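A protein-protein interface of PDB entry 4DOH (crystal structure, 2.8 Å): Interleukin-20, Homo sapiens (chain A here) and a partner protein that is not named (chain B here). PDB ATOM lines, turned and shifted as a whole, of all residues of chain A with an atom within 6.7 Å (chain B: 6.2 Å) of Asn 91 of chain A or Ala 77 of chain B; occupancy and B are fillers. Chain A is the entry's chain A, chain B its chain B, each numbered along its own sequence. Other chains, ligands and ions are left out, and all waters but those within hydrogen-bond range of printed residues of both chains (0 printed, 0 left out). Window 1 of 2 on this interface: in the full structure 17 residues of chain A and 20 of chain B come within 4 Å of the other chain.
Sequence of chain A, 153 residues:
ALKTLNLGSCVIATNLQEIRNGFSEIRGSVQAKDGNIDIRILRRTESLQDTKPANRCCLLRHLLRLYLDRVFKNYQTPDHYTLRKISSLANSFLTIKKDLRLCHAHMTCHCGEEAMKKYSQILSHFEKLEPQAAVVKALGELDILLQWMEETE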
ATOM      1  N   GLU A  18      17.328   7.601   5.548  1.00  0.00           N
ATOM      2  CA  GLU A  18      18.348   8.087   6.466  1.00  0.00           C
ATOM      3  C   GLU A  18      18.928   6.941   7.283  1.00  0.00           C
ATOM      4  O   GLU A  18      20.137   6.771   7.343  1.00  0.00           O
ATOM      5  CB  GLU A  18      17.764   9.158   7.384  1.00  0.00           C
ATOM      6  CG  GLU A  18      18.772   9.924   8.236  1.00  0.00           C
ATOM      7  CD  GLU A  18      18.135  11.108   8.975  1.00  0.00           C
ATOM      8  OE1 GLU A  18      17.240  10.878   9.832  1.00  0.00           O
ATOM      9  OE2 GLU A  18      18.527  12.270   8.692  1.00  0.00           O
ATOM     10  N   LEU A  68      16.255   0.523  21.897  1.00  0.00           N
ATOM     11  CA  LEU A  68      16.622   1.746  22.599  1.00  0.00           C
ATOM     12  C   LEU A  68      17.015   1.475  24.059  1.00  0.00           C
ATOM     13  O   LEU A  68      17.885   2.153  24.595  1.00  0.00           O
ATOM     14  CB  LEU A  68      15.488   2.769  22.533  1.00  0.00           C
ATOM     15  CG  LEU A  68      15.096   3.317  21.174  1.00  0.00           C
ATOM     16  CD1 LEU A  68      13.719   3.978  21.243  1.00  0.00           C
ATOM     17  CD2 LEU A  68      16.128   4.298  20.714  1.00  0.00           C
ATOM     18  N   PHE A  72      21.537  -0.048  21.350  1.00  0.00           N
ATOM     19  CA  PHE A  72      22.344   1.105  20.956  1.00  0.00           C
ATOM     20  C   PHE A  72      23.334   1.615  22.005  1.00  0.00           C
ATOM     21  O   PHE A  72      24.507   1.796  21.697  1.00  0.00           O
ATOM     22  CB  PHE A  72      21.456   2.253  20.454  1.00  0.00           C
ATOM     23  CG  PHE A  72      20.649   1.900  19.250  1.00  0.00           C
ATOM     24  CD1 PHE A  72      21.264   1.392  18.111  1.00  0.00           C
ATOM     25  CD2 PHE A  72      19.267   2.047  19.257  1.00  0.00           C
ATOM     26  CE1 PHE A  72      20.518   1.036  16.993  1.00  0.00           C
ATOM     27  CE2 PHE A  72      18.515   1.717  18.142  1.00  0.00           C
ATOM     28  CZ  PHE A  72      19.149   1.201  17.007  1.00  0.00           C
ATOM     29  N   ILE A  86      26.203   5.050  15.399  1.00  0.00           N
ATOM     30  CA  ILE A  86      25.258   4.393  16.276  1.00  0.00           C
ATOM     31  C   ILE A  86      24.365   5.430  16.967  1.00  0.00           C
ATOM     32  O   ILE A  86      23.172   5.206  17.166  1.00  0.00           O
ATOM     33  CB  ILE A  86      25.964   3.419  17.256  1.00  0.00           C
ATOM     34  CG1 ILE A  86      26.463   2.185  16.483  1.00  0.00           C
ATOM     35  CG2 ILE A  86      25.028   2.997  18.404  1.00  0.00           C
ATOM     36  CD1 ILE A  86      27.519   1.373  17.211  1.00  0.00           C
ATOM     37  N   SER A  87      24.926   6.588  17.282  1.00  0.00           N
ATOM     38  CA  SER A  87      24.125   7.663  17.857  1.00  0.00           C
ATOM     39  C   SER A  87      23.077   8.135  16.841  1.00  0.00           C
ATOM     40  O   SER A  87      21.956   8.514  17.195  1.00  0.00           O
ATOM     41  CB  SER A  87      25.012   8.836  18.280  1.00  0.00           C
ATOM     42  OG  SER A  87      24.240   9.843  18.907  1.00  0.00           O
ATOM     43  N   SER A  88      23.455   8.111  15.571  1.00  0.00           N
ATOM     44  CA  SER A  88      22.543   8.516  14.523  1.00  0.00           C
ATOM     45  C   SER A  88      21.388   7.557  14.498  1.00  0.00           C
ATOM     46  O   SER A  88      20.232   7.971  14.555  1.00  0.00           O
ATOM     47  CB  SER A  88      23.226   8.501  13.161  1.00  0.00           C
ATOM     48  OG  SER A  88      24.223   9.502  13.087  1.00  0.00           O
ATOM     49  N   LEU A  89      21.711   6.269  14.406  1.00  0.00           N
ATOM     50  CA  LEU A  89      20.683   5.262  14.353  1.00  0.00           C
ATOM     51  C   LEU A  89      19.721   5.405  15.546  1.00  0.00           C
ATOM     52  O   LEU A  89      18.496   5.413  15.378  1.00  0.00           O
ATOM     53  CB  LEU A  89      21.306   3.875  14.304  1.00  0.00           C
ATOM     54  CG  LEU A  89      22.149   3.535  13.081  1.00  0.00           C
ATOM     55  CD1 LEU A  89      22.708   2.143  13.224  1.00  0.00           C
ATOM     56  CD2 LEU A  89      21.303   3.599  11.870  1.00  0.00           C
ATOM     57  N   ALA A  90      20.277   5.547  16.742  1.00  0.00           N
ATOM     58  CA  ALA A  90      19.448   5.580  17.920  1.00  0.00           C
ATOM     59  C   ALA A  90      18.540   6.809  17.956  1.00  0.00           C
ATOM     60  O   ALA A  90      17.377   6.716  18.348  1.00  0.00           O
ATOM     61  CB  ALA A  90      20.293   5.472  19.202  1.00  0.00           C
ATOM     62  N   ASN A  91      19.053   7.962  17.560  1.00  0.00           N
ATOM     63  CA  ASN A  91      18.232   9.155  17.628  1.00  0.00           C
ATOM     64  C   ASN A  91      17.152   9.113  16.547  1.00  0.00           C
ATOM     65  O   ASN A  91      16.018   9.546  16.758  1.00  0.00           O
ATOM     66  CB  ASN A  91      19.094  10.414  17.520  1.00  0.00           C
ATOM     67  CG  ASN A  91      19.801  10.734  18.807  1.00  0.00           C
ATOM     68  OD1 ASN A  91      19.222  11.330  19.705  1.00  0.00           O
ATOM     69  ND2 ASN A  91      21.052  10.328  18.915  1.00  0.00           N
ATOM     70  N   SER A  92      17.514   8.578  15.386  1.00  0.00           N
ATOM     71  CA  SER A  92      16.557   8.334  14.329  1.00  0.00           C
ATOM     72  C   SER A  92      15.477   7.379  14.829  1.00  0.00           C
ATOM     73  O   SER A  92      14.275   7.601  14.569  1.00  0.00           O
ATOM     74  CB  SER A  92      17.240   7.768  13.085  1.00  0.00           C
ATOM     75  OG  SER A  92      18.020   8.760  12.428  1.00  0.00           O
ATOM     76  N   PHE A  93      15.885   6.328  15.554  1.00  0.00           N
ATOM     77  CA  PHE A  93      14.898   5.389  16.094  1.00  0.00           C
ATOM     78  C   PHE A  93      14.004   6.033  17.116  1.00  0.00           C
ATOM     79  O   PHE A  93      12.855   5.650  17.270  1.00  0.00           O
ATOM     80  CB  PHE A  93      15.532   4.130  16.656  1.00  0.00           C
ATOM     81  CG  PHE A  93      15.686   3.060  15.641  1.00  0.00           C
ATOM     82  CD1 PHE A  93      16.904   2.782  15.095  1.00  0.00           C
ATOM     83  CD2 PHE A  93      14.594   2.387  15.175  1.00  0.00           C
ATOM     84  CE1 PHE A  93      17.038   1.816  14.129  1.00  0.00           C
ATOM     85  CE2 PHE A  93      14.729   1.418  14.207  1.00  0.00           C
ATOM     86  CZ  PHE A  93      15.959   1.133  13.692  1.00  0.00           C
ATOM     87  N   LEU A  94      14.539   7.032  17.790  1.00  0.00           N
ATOM     88  CA  LEU A  94      13.816   7.738  18.828  1.00  0.00           C
ATOM     89  C   LEU A  94      12.661   8.583  18.251  1.00  0.00           C
ATOM     90  O   LEU A  94      11.600   8.704  18.849  1.00  0.00           O
ATOM     91  CB  LEU A  94      14.800   8.629  19.584  1.00  0.00           C
ATOM     92  CG  LEU A  94      14.207   9.285  20.814  1.00  0.00           C
ATOM     93  CD1 LEU A  94      13.826   8.192  21.765  1.00  0.00           C
ATOM     94  CD2 LEU A  94      15.187  10.263  21.448  1.00  0.00           C
ATOM     95  N   THR A  95      12.863   9.185  17.090  1.00  0.00           N
ATOM     96  CA  THR A  95      11.787   9.963  16.506  1.00  0.00           C
ATOM     97  C   THR A  95      10.618   9.033  16.210  1.00  0.00           C
ATOM     98  O   THR A  95       9.467   9.411  16.340  1.00  0.00           O
ATOM     99  CB  THR A  95      12.211  10.723  15.208  1.00  0.00           C
ATOM    100  OG1 THR A  95      12.515   9.785  14.172  1.00  0.00           O
ATOM    101  CG2 THR A  95      13.442  11.633  15.452  1.00  0.00           C
ATOM    102  N   ILE A  96      10.918   7.809  15.810  1.00  0.00           N
ATOM    103  CA  ILE A  96       9.875   6.856  15.505  1.00  0.00           C
ATOM    104  C   ILE A  96       9.167   6.407  16.778  1.00  0.00           C
ATOM    105  O   ILE A  96       7.948   6.329  16.805  1.00  0.00           O
ATOM    106  CB  ILE A  96      10.433   5.622  14.771  1.00  0.00           C
ATOM    107  CG1 ILE A  96      11.184   6.026  13.499  1.00  0.00           C
ATOM    108  CG2 ILE A  96       9.322   4.639  14.453  1.00  0.00           C
ATOM    109  CD1 ILE A  96      11.907   4.836  12.811  1.00  0.00           C
ATOM    110  N   GLN B  43      25.473  15.705  22.278  1.00  0.00           N
ATOM    111  CA  GLN B  43      24.636  14.582  22.635  1.00  0.00           C
ATOM    112  C   GLN B  43      23.239  14.816  22.105  1.00  0.00           C
ATOM    113  O   GLN B  43      22.670  15.893  22.259  1.00  0.00           O
ATOM    114  CB  GLN B  43      24.662  14.281  24.153  1.00  0.00           C
ATOM    115  CG  GLN B  43      23.959  15.284  25.065  1.00  0.00           C
ATOM    116  CD  GLN B  43      23.995  14.867  26.529  1.00  0.00           C
ATOM    117  OE1 GLN B  43      24.765  13.979  26.916  1.00  0.00           O
ATOM    118  NE2 GLN B  43      23.156  15.503  27.349  1.00  0.00           N
ATOM    119  N   GLY B  44      22.717  13.800  21.434  1.00  0.00           N
ATOM    120  CA  GLY B  44      21.362  13.820  20.939  1.00  0.00           C
ATOM    121  C   GLY B  44      20.426  13.482  22.071  1.00  0.00           C
ATOM    122  O   GLY B  44      20.857  12.945  23.093  1.00  0.00           O
ATOM    123  N   GLU B  45      19.149  13.801  21.886  1.00  0.00           N
ATOM    124  CA  GLU B  45      18.117  13.473  22.858  1.00  0.00           C
ATOM    125  C   GLU B  45      18.198  12.040  23.376  1.00  0.00           C
ATOM    126  O   GLU B  45      17.923  11.799  24.547  1.00  0.00           O
ATOM    127  CB  GLU B  45      16.749  13.724  22.250  1.00  0.00           C
ATOM    128  CG  GLU B  45      15.591  13.278  23.118  1.00  0.00           C
ATOM    129  CD  GLU B  45      14.308  13.997  22.750  1.00  0.00           C
ATOM    130  OE1 GLU B  45      13.657  13.604  21.748  1.00  0.00           O
ATOM    131  OE2 GLU B  45      13.964  14.967  23.461  1.00  0.00           O
ATOM    132  N   TYR B  46      18.573  11.091  22.520  1.00  0.00           N
ATOM    133  CA  TYR B  46      18.785   9.721  22.987  1.00  0.00           C
ATOM    134  C   TYR B  46      19.782   9.662  24.136  1.00  0.00           C
ATOM    135  O   TYR B  46      19.521   9.071  25.176  1.00  0.00           O
ATOM    136  CB  TYR B  46      19.278   8.804  21.871  1.00  0.00           C
ATOM    137  CG  TYR B  46      19.540   7.391  22.355  1.00  0.00           C
ATOM    138  CD1 TYR B  46      18.488   6.584  22.785  1.00  0.00           C
ATOM    139  CD2 TYR B  46      20.833   6.862  22.389  1.00  0.00           C
ATOM    140  CE1 TYR B  46      18.708   5.292  23.238  1.00  0.00           C
ATOM    141  CE2 TYR B  46      21.068   5.558  22.830  1.00  0.00           C
ATOM    142  CZ  TYR B  46      19.995   4.785  23.257  1.00  0.00           C
ATOM    143  OH  TYR B  46      20.198   3.500  23.701  1.00  0.00           O
ATOM    144  N   GLU B  47      20.934  10.277  23.923  1.00  0.00           N
ATOM    145  CA  GLU B  47      21.996  10.306  24.911  1.00  0.00           C
ATOM    146  C   GLU B  47      21.553  11.067  26.150  1.00  0.00           C
ATOM    147  O   GLU B  47      21.807  10.639  27.268  1.00  0.00           O
ATOM    148  CB  GLU B  47      23.241  10.948  24.313  1.00  0.00           C
ATOM    149  CG  GLU B  47      23.976  10.068  23.311  1.00  0.00           C
ATOM    150  CD  GLU B  47      23.345  10.051  21.917  1.00  0.00           C
ATOM    151  OE1 GLU B  47      22.577  10.978  21.558  1.00  0.00           O
ATOM    152  OE2 GLU B  47      23.626   9.094  21.166  1.00  0.00           O
ATOM    153  N   ASP B  74      27.048  15.645  12.287  1.00  0.00           N
ATOM    154  CA  ASP B  74      26.765  15.178  13.640  1.00  0.00           C
ATOM    155  C   ASP B  74      25.263  15.183  13.955  1.00  0.00           C
ATOM    156  O   ASP B  74      24.738  14.218  14.514  1.00  0.00           O
ATOM    157  CB  ASP B  74      27.539  16.029  14.670  1.00  0.00           C
ATOM    158  CG  ASP B  74      29.058  15.770  14.644  1.00  0.00           C
ATOM    159  OD1 ASP B  74      29.454  14.586  14.503  1.00  0.00           O
ATOM    160  OD2 ASP B  74      29.855  16.743  14.777  1.00  0.00           O
ATOM    161  N   ILE B  75      24.589  16.277  13.606  1.00  0.00           N
ATOM    162  CA  ILE B  75      23.149  16.420  13.806  1.00  0.00           C
ATOM    163  C   ILE B  75      22.384  15.686  12.700  1.00  0.00           C
ATOM    164  O   ILE B  75      22.037  16.265  11.668  1.00  0.00           O
ATOM    165  CB  ILE B  75      22.730  17.901  13.782  1.00  0.00           C
ATOM    166  CG1 ILE B  75      23.213  18.628  15.031  1.00  0.00           C
ATOM    167  CG2 ILE B  75      21.209  18.038  13.671  1.00  0.00           C
ATOM    168  CD1 ILE B  75      24.661  18.574  15.222  1.00  0.00           C
ATOM    169  N   THR B  76      22.107  14.408  12.916  1.00  0.00           N
ATOM    170  CA  THR B  76      21.623  13.564  11.830  1.00  0.00           C
ATOM    171  C   THR B  76      20.258  12.975  12.123  1.00  0.00           C
ATOM    172  O   THR B  76      19.854  11.991  11.507  1.00  0.00           O
ATOM    173  CB  THR B  76      22.570  12.382  11.604  1.00  0.00           C
ATOM    174  OG1 THR B  76      22.669  11.624  12.817  1.00  0.00           O
ATOM    175  CG2 THR B  76      23.937  12.862  11.205  1.00  0.00           C
ATOM    176  N   ALA B  77      19.561  13.562  13.081  1.00  0.00           N
ATOM    177  CA  ALA B  77      18.244  13.088  13.449  1.00  0.00           C
ATOM    178  C   ALA B  77      17.421  14.296  13.881  1.00  0.00           C
ATOM    179  O   ALA B  77      17.990  15.286  14.364  1.00  0.00           O
ATOM    180  CB  ALA B  77      18.339  12.059  14.570  1.00  0.00           C
ATOM    181  N   THR B  78      16.098  14.237  13.699  1.00  0.00           N
ATOM    182  CA  THR B  78      15.286  15.408  13.992  1.00  0.00           C
ATOM    183  C   THR B  78      14.831  15.452  15.454  1.00  0.00           C
ATOM    184  O   THR B  78      13.657  15.331  15.774  1.00  0.00           O
ATOM    185  CB  THR B  78      14.150  15.611  12.977  1.00  0.00           C
ATOM    186  OG1 THR B  78      14.663  15.400  11.659  1.00  0.00           O
ATOM    187  CG2 THR B  78      13.617  17.038  13.045  1.00  0.00           C
ATOM    188  N   VAL B  79      15.819  15.637  16.325  1.00  0.00           N
ATOM    189  CA  VAL B  79      15.640  15.748  17.763  1.00  0.00           C
ATOM    190  C   VAL B  79      16.508  16.888  18.283  1.00  0.00           C
ATOM    191  O   VAL B  79      17.402  17.362  17.579  1.00  0.00           O
ATOM    192  CB  VAL B  79      16.051  14.459  18.462  1.00  0.00           C
ATOM    193  CG1 VAL B  79      15.192  13.325  17.968  1.00  0.00           C
ATOM    194  CG2 VAL B  79      17.543  14.170  18.232  1.00  0.00           C
ATOM    195  N   PRO B  80      16.224  17.366  19.502  1.00  0.00           N
ATOM    196  CA  PRO B  80      17.062  18.398  20.112  1.00  0.00           C
ATOM    197  C   PRO B  80      18.425  17.829  20.431  1.00  0.00           C
ATOM    198  O   PRO B  80      18.525  16.714  20.936  1.00  0.00           O
ATOM    199  CB  PRO B  80      16.325  18.715  21.412  1.00  0.00           C
ATOM    200  CG  PRO B  80      15.555  17.477  21.708  1.00  0.00           C
ATOM    201  CD  PRO B  80      15.091  17.008  20.373  1.00  0.00           C
ATOM    202  N   TYR B  81      19.464  18.588  20.116  1.00  0.00           N
ATOM    203  CA  TYR B  81      20.812  18.156  20.406  1.00  0.00           C
ATOM    204  C   TYR B  81      21.408  19.091  21.415  1.00  0.00           C
ATOM    205  O   TYR B  81      21.108  20.281  21.407  1.00  0.00           O
ATOM    206  CB  TYR B  81      21.665  18.189  19.150  1.00  0.00           C
ATOM    207  CG  TYR B  81      21.597  16.945  18.315  1.00  0.00           C
ATOM    208  CD1 TYR B  81      20.463  16.633  17.597  1.00  0.00           C
ATOM    209  CD2 TYR B  81      22.676  16.099  18.226  1.00  0.00           C
ATOM    210  CE1 TYR B  81      20.407  15.498  16.818  1.00  0.00           C
ATOM    211  CE2 TYR B  81      22.633  14.977  17.458  1.00  0.00           C
ATOM    212  CZ  TYR B  81      21.501  14.672  16.747  1.00  0.00           C
ATOM    213  OH  TYR B  81      21.464  13.530  15.967  1.00  0.00           O
ATOM    214  N   ASN B 104      17.685  22.015  17.419  1.00  0.00           N
ATOM    215  CA  ASN B 104      16.972  21.070  16.553  1.00  0.00           C
ATOM    216  C   ASN B 104      16.996  21.495  15.081  1.00  0.00           C
ATOM    217  O   ASN B 104      16.595  22.608  14.752  1.00  0.00           O
ATOM    218  CB  ASN B 104      15.523  20.918  16.996  1.00  0.00           C
ATOM    219  CG  ASN B 104      14.860  19.692  16.399  1.00  0.00           C
ATOM    220  OD1 ASN B 104      15.150  19.300  15.277  1.00  0.00           O
ATOM    221  ND2 ASN B 104      13.973  19.076  17.159  1.00  0.00           N
ATOM    222  N   ARG B 105      17.442  20.612  14.196  1.00  0.00           N
ATOM    223  CA  ARG B 105      17.609  21.002  12.797  1.00  0.00           C
ATOM    224  C   ARG B 105      16.316  21.501  12.146  1.00  0.00           C
ATOM    225  O   ARG B 105      16.350  22.148  11.087  1.00  0.00           O
ATOM    226  CB  ARG B 105      18.235  19.880  11.978  1.00  0.00           C
ATOM    227  CG  ARG B 105      17.340  18.674  11.774  1.00  0.00           C
ATOM    228  CD  ARG B 105      18.116  17.598  11.037  1.00  0.00           C
ATOM    229  NE  ARG B 105      17.412  16.333  11.046  1.00  0.00           N
ATOM    230  CZ  ARG B 105      17.880  15.225  10.495  1.00  0.00           C
ATOM    231  NH1 ARG B 105      19.069  15.215   9.900  1.00  0.00           N
ATOM    232  NH2 ARG B 105      17.158  14.122  10.548  1.00  0.00           N
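OD1 of Asn 91 of chain A sits at hydrogen-bond distance from N of Tyr 46 of chain B, at 2.9 Å.
O of Leu 68 of chain A lies within hydrogen-bond range of OH of Tyr 46 of chain B (2.8 Å).
The side-chain carboxylate (OE1) of Glu 47 of chain B sits at hydrogen-bond distance from the side-chain amide nitrogen (ND2) of Asn 91 of chain A, 3.1 Å away.
OD1 of Asn 91 of chain A lies within hydrogen-bond range of N of Glu 45 of chain B (3.3 Å).
OE2 of Glu 18 of chain A lies within salt-bridge range of NH2 of Arg 105 of chain B, 3.0 Å away.
The side-chain carboxylate (OE2) of Glu 18 of chain A sits close to the backbone carbonyl oxygen (O) of Thr 76 of chain B (3.1 Å).
The side-chain hydroxyl (OG) of Ser 87 of chain A is in hydrogen-bond range of the side-chain carboxylate (OE2) of Glu 47 of chain B.
The side-chain hydroxyl (OG) of Ser 88 of chain A is in hydrogen-bond range of the side-chain hydroxyl (OG1) of Thr 76 of chain B.
The side-chain carboxylate (OE1) of Glu 47 of chain B lies within hydrogen-bond range of the backbone NH (N) of Gly 44 of chain B (2.8 Å).
The backbone NH (N) of Thr 76 of chain B is in hydrogen-bond range of the side-chain hydroxyl (OH) of Tyr 81 of chain B, at 3.2 Å.
N of Ala 77 of chain B is in hydrogen-bond range of OH of Tyr 81 of chain B (3.5 Å).
O of Ser 88 of chain A lies within hydrogen-bond range of OG of Ser 92 of chain A (3.2 Å).
O of Ser 92 of chain A sits at hydrogen-bond distance from OG1 of Thr 95 of chain A (2.8 Å).
The side-chain carboxylate of Glu 18 of chain A sits at hydrogen-bond distance from the side-chain hydroxyl of Ser 92 of chain A, at 3.4 Å.
Among the printed residues, pairs that only touch across the chains: Asn 91 of chain A with Gly 44 of chain B (3.4 Å), Asn 91 of chain A with Ala 77 of chain B (3.5 Å), Leu 94 of chain A with Glu 45 of chain B (3.5 Å), Thr 95 of chain A with Val 79 of chain B (3.5 Å), Ala 90 of chain A with Tyr 46 of chain B (3.5 Å), Asn 91 of chain A with Val 79 of chain B (3.6 Å), Leu 94 of chain A with Tyr 46 of chain B (3.6 Å), Ser 92 of chain A with Ala 77 of chain B (3.7 Å), Phe 72 of chain A with Tyr 46 of chain B (3.7 Å), Thr 95 of chain A with Thr 78 of chain B (3.7 Å) and Ser 92 of chain A with Thr 76 of chain B (3.8 Å).
Of the printed residues of chain B, Leu 68 of chain A touches Tyr 46 (2.8 Å).
Of the printed residues of chain B, Phe 72 of chain A touches Tyr 46.
Of the printed residues of chain B, Ala 90 of chain A touches Tyr 46 (3.5 Å).
Of the printed residues of chain A, Gly 44 of chain B touches Asn 91.
Ile 75 of chain B touches none of the printed residues of chain A.
Ala 77 of chain B touches just these residues of chain A: Asn 91 (3.5 Å) and Ser 92 (3.7 Å).
Printed residues of chain A within 4 Å of Arg 105 of chain B: Glu 18.
The nearest residue of chain A that does not touch Ala 77 of chain B is Glu 18 of chain A (4.4 Å).
Hydrophobic or aromatic side chains of chain B within 4 Å of the printed part of chain A: Tyr 46, Ala 77 and Val 79.
Of the 14 printed residues of chain A, 10 touch a printed residue of chain B.
Hydrophobic or aromatic side chains of chain A that line the printed part of chain B: Leu 68, Phe 72, Ala 90 and Leu 94.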
